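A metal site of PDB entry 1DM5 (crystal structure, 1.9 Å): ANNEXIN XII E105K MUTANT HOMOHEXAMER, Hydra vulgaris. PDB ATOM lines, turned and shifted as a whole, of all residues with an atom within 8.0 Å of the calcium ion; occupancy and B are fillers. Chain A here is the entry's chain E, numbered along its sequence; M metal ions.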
ATOM      1  N   ILE A 176       1.316  11.703  -1.929  1.00  0.00           N
ATOM      2  CA  ILE A 176       0.873  10.310  -1.910  1.00  0.00           C
ATOM      3  C   ILE A 176      -0.527  10.158  -2.489  1.00  0.00           C
ATOM      4  O   ILE A 176      -0.817   9.186  -3.186  1.00  0.00           O
ATOM      5  CB  ILE A 176       0.921   9.757  -0.477  1.00  0.00           C
ATOM      6  CG1 ILE A 176       2.353   9.629   0.057  1.00  0.00           C
ATOM      7  CG2 ILE A 176       0.172   8.435  -0.380  1.00  0.00           C
ATOM      8  CD1 ILE A 176       2.417   9.244   1.513  1.00  0.00           C
ATOM      9  N   TYR A 177      -1.363  11.159  -2.261  1.00  0.00           N
ATOM     10  CA  TYR A 177      -2.693  11.195  -2.866  1.00  0.00           C
ATOM     11  C   TYR A 177      -2.589  11.223  -4.386  1.00  0.00           C
ATOM     12  O   TYR A 177      -3.220  10.433  -5.075  1.00  0.00           O
ATOM     13  CB  TYR A 177      -3.466  12.440  -2.403  1.00  0.00           C
ATOM     14  CG  TYR A 177      -4.910  12.433  -2.851  1.00  0.00           C
ATOM     15  CD1 TYR A 177      -5.880  11.749  -2.146  1.00  0.00           C
ATOM     16  CD2 TYR A 177      -5.295  13.119  -3.998  1.00  0.00           C
ATOM     17  CE1 TYR A 177      -7.195  11.736  -2.548  1.00  0.00           C
ATOM     18  CE2 TYR A 177      -6.617  13.118  -4.415  1.00  0.00           C
ATOM     19  CZ  TYR A 177      -7.554  12.432  -3.685  1.00  0.00           C
ATOM     20  OH  TYR A 177      -8.866  12.431  -4.106  1.00  0.00           O
ATOM     21  N   GLN A 178      -1.801  12.171  -4.892  1.00  0.00           N
ATOM     22  CA  GLN A 178      -1.698  12.378  -6.327  1.00  0.00           C
ATOM     23  C   GLN A 178      -1.089  11.162  -7.010  1.00  0.00           C
ATOM     24  O   GLN A 178      -1.457  10.839  -8.136  1.00  0.00           O
ATOM     25  CB  GLN A 178      -0.900  13.644  -6.664  1.00  0.00           C
ATOM     26  CG  GLN A 178      -1.286  14.862  -5.846  1.00  0.00           C
ATOM     27  CD  GLN A 178      -2.602  15.485  -6.234  1.00  0.00           C
ATOM     28  OE1 GLN A 178      -2.766  16.710  -6.128  1.00  0.00           O
ATOM     29  NE2 GLN A 178      -3.561  14.675  -6.675  1.00  0.00           N
ATOM     30  N   ALA A 179      -0.194  10.499  -6.292  1.00  0.00           N
ATOM     31  CA  ALA A 179       0.499   9.310  -6.782  1.00  0.00           C
ATOM     32  C   ALA A 179      -0.375   8.074  -6.790  1.00  0.00           C
ATOM     33  O   ALA A 179      -0.059   7.080  -7.453  1.00  0.00           O
ATOM     34  CB  ALA A 179       1.726   9.045  -5.906  1.00  0.00           C
ATOM     35  N   GLY A 180      -1.475   8.076  -6.036  1.00  0.00           N
ATOM     36  CA  GLY A 180      -2.303   6.881  -5.960  1.00  0.00           C
ATOM     37  C   GLY A 180      -3.764   7.160  -6.254  1.00  0.00           C
ATOM     38  O   GLY A 180      -4.259   6.819  -7.321  1.00  0.00           O
ATOM     39  N   GLU A 181      -4.466   7.777  -5.300  1.00  0.00           N
ATOM     40  CA  GLU A 181      -5.888   8.033  -5.506  1.00  0.00           C
ATOM     41  C   GLU A 181      -6.168   8.967  -6.671  1.00  0.00           C
ATOM     42  O   GLU A 181      -7.054   8.694  -7.482  1.00  0.00           O
ATOM     43  CB  GLU A 181      -6.522   8.589  -4.231  1.00  0.00           C
ATOM     44  CG  GLU A 181      -6.869   7.476  -3.234  1.00  0.00           C
ATOM     45  CD  GLU A 181      -7.731   8.013  -2.105  1.00  0.00           C
ATOM     46  OE1 GLU A 181      -7.168   8.467  -1.099  1.00  0.00           O
ATOM     47  OE2 GLU A 181      -8.975   7.987  -2.273  1.00  0.00           O
ATOM     48  N   GLY A 182      -5.429  10.064  -6.733  1.00  0.00           N
ATOM     49  CA  GLY A 182      -5.606  11.128  -7.681  1.00  0.00           C
ATOM     50  C   GLY A 182      -5.328  10.799  -9.127  1.00  0.00           C
ATOM     51  O   GLY A 182      -5.441  11.684  -9.992  1.00  0.00           O
ATOM     52  N   GLN A 183      -4.957   9.552  -9.460  1.00  0.00           N
ATOM     53  CA  GLN A 183      -4.723   9.279 -10.879  1.00  0.00           C
ATOM     54  C   GLN A 183      -5.206   7.904 -11.272  1.00  0.00           C
ATOM     55  O   GLN A 183      -5.560   7.089 -10.421  1.00  0.00           O
ATOM     56  CB  GLN A 183      -3.256   9.507 -11.257  1.00  0.00           C
ATOM     57  CG  GLN A 183      -2.226   8.638 -10.569  1.00  0.00           C
ATOM     58  CD  GLN A 183      -0.934   8.546 -11.363  1.00  0.00           C
ATOM     59  OE1 GLN A 183      -0.775   7.677 -12.224  1.00  0.00           O
ATOM     60  NE2 GLN A 183      -0.003   9.461 -11.127  1.00  0.00           N
ATOM     61  N   ILE A 184      -5.250   7.643 -12.578  1.00  0.00           N
ATOM     62  CA  ILE A 184      -5.660   6.339 -13.098  1.00  0.00           C
ATOM     63  C   ILE A 184      -4.611   5.283 -12.775  1.00  0.00           C
ATOM     64  O   ILE A 184      -4.914   4.207 -12.269  1.00  0.00           O
ATOM     65  CB  ILE A 184      -5.886   6.362 -14.621  1.00  0.00           C
ATOM     66  CG1 ILE A 184      -6.796   7.472 -15.146  1.00  0.00           C
ATOM     67  CG2 ILE A 184      -6.392   4.994 -15.067  1.00  0.00           C
ATOM     68  CD1 ILE A 184      -8.081   6.983 -15.760  1.00  0.00           C
ATOM     69  N   GLY A 185      -3.352   5.589 -13.073  1.00  0.00           N
ATOM     70  CA  GLY A 185      -2.248   4.719 -12.713  1.00  0.00           C
ATOM     71  C   GLY A 185      -1.667   5.062 -11.350  1.00  0.00           C
ATOM     72  O   GLY A 185      -2.234   5.834 -10.577  1.00  0.00           O
ATOM     73  N   THR A 186      -0.512   4.475 -11.051  1.00  0.00           N
ATOM     74  CA  THR A 186       0.102   4.650  -9.749  1.00  0.00           C
ATOM     75  C   THR A 186       1.551   5.101  -9.831  1.00  0.00           C
ATOM     76  O   THR A 186       2.296   4.598 -10.679  1.00  0.00           O
ATOM     77  CB  THR A 186       0.066   3.309  -8.981  1.00  0.00           C
ATOM     78  OG1 THR A 186      -1.293   2.834  -8.920  1.00  0.00           O
ATOM     79  CG2 THR A 186       0.537   3.500  -7.556  1.00  0.00           C
ATOM     80  N   ASP A 187       1.985   5.949  -8.916  1.00  0.00           N
ATOM     81  CA  ASP A 187       3.410   6.146  -8.673  1.00  0.00           C
ATOM     82  C   ASP A 187       3.776   5.433  -7.373  1.00  0.00           C
ATOM     83  O   ASP A 187       3.767   6.023  -6.291  1.00  0.00           O
ATOM     84  CB  ASP A 187       3.815   7.606  -8.576  1.00  0.00           C
ATOM     85  CG  ASP A 187       5.325   7.802  -8.610  1.00  0.00           C
ATOM     86  OD1 ASP A 187       5.744   8.977  -8.722  1.00  0.00           O
ATOM     87  OD2 ASP A 187       6.081   6.818  -8.549  1.00  0.00           O
ATOM     88  N   PHE A 191       5.074   6.238  -2.847  1.00  0.00           N
ATOM     89  CA  PHE A 191       4.716   5.557  -1.601  1.00  0.00           C
ATOM     90  C   PHE A 191       5.986   5.062  -0.914  1.00  0.00           C
ATOM     91  O   PHE A 191       6.151   5.123   0.305  1.00  0.00           O
ATOM     92  CB  PHE A 191       3.793   4.359  -1.888  1.00  0.00           C
ATOM     93  CG  PHE A 191       2.339   4.730  -2.135  1.00  0.00           C
ATOM     94  CD1 PHE A 191       1.395   4.598  -1.135  1.00  0.00           C
ATOM     95  CD2 PHE A 191       1.919   5.189  -3.375  1.00  0.00           C
ATOM     96  CE1 PHE A 191       0.073   4.939  -1.358  1.00  0.00           C
ATOM     97  CE2 PHE A 191       0.609   5.528  -3.619  1.00  0.00           C
ATOM     98  CZ  PHE A 191      -0.329   5.398  -2.607  1.00  0.00           C
ATOM     99  N   ASN A 224      -6.371  -0.332  -1.616  1.00  0.00           N
ATOM    100  CA  ASN A 224      -7.037  -0.158  -2.889  1.00  0.00           C
ATOM    101  C   ASN A 224      -6.075   0.051  -4.039  1.00  0.00           C
ATOM    102  O   ASN A 224      -6.377  -0.284  -5.191  1.00  0.00           O
ATOM    103  CB  ASN A 224      -7.993   1.044  -2.768  1.00  0.00           C
ATOM    104  CG  ASN A 224      -9.201   0.936  -3.679  1.00  0.00           C
ATOM    105  OD1 ASN A 224     -10.239   0.399  -3.291  1.00  0.00           O
ATOM    106  ND2 ASN A 224      -9.066   1.446  -4.897  1.00  0.00           N
ATOM    107  N   GLU A 225      -4.903   0.624  -3.775  1.00  0.00           N
ATOM    108  CA  GLU A 225      -3.977   0.917  -4.851  1.00  0.00           C
ATOM    109  C   GLU A 225      -3.082  -0.241  -5.255  1.00  0.00           C
ATOM    110  O   GLU A 225      -2.693  -0.313  -6.435  1.00  0.00           O
ATOM    111  CB  GLU A 225      -3.143   2.151  -4.491  1.00  0.00           C
ATOM    112  CG  GLU A 225      -2.456   2.760  -5.716  1.00  0.00           C
ATOM    113  CD  GLU A 225      -3.442   3.538  -6.558  1.00  0.00           C
ATOM    114  OE1 GLU A 225      -4.567   3.789  -6.069  1.00  0.00           O
ATOM    115  OE2 GLU A 225      -3.090   3.889  -7.694  1.00  0.00           O
HETATM  116 CA    CA M   1      -4.312   5.440  -9.092  1.00  0.00          CA
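OE1 of Gln 183 sits at hydrogen-bond distance from N of Thr 186, at 3.4 Å. OE2 of Glu 225 sits close to OG1 of Thr 186, 2.4 Å away. OE1 of Gln 183 sits close to N of Gly 185 (3.4 Å).
O of Ile 184 touches the calcium ion (3.5 Å). Thr 186 touches the calcium ion (OG1 to CA, 3.99 Å).
The calcium ion is bound by the backbone carbonyl oxygen (O) of Gly 180 (2.2 Å), the side-chain carboxylate (OE2) of Glu 225 (2.4 Å), the backbone carbonyl oxygen (O) of Gln 183 (2.5 Å) and the backbone carbonyl oxygen (O) of Gly 185 (2.6 Å). The calcium ion has four donor atoms within binding distance.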
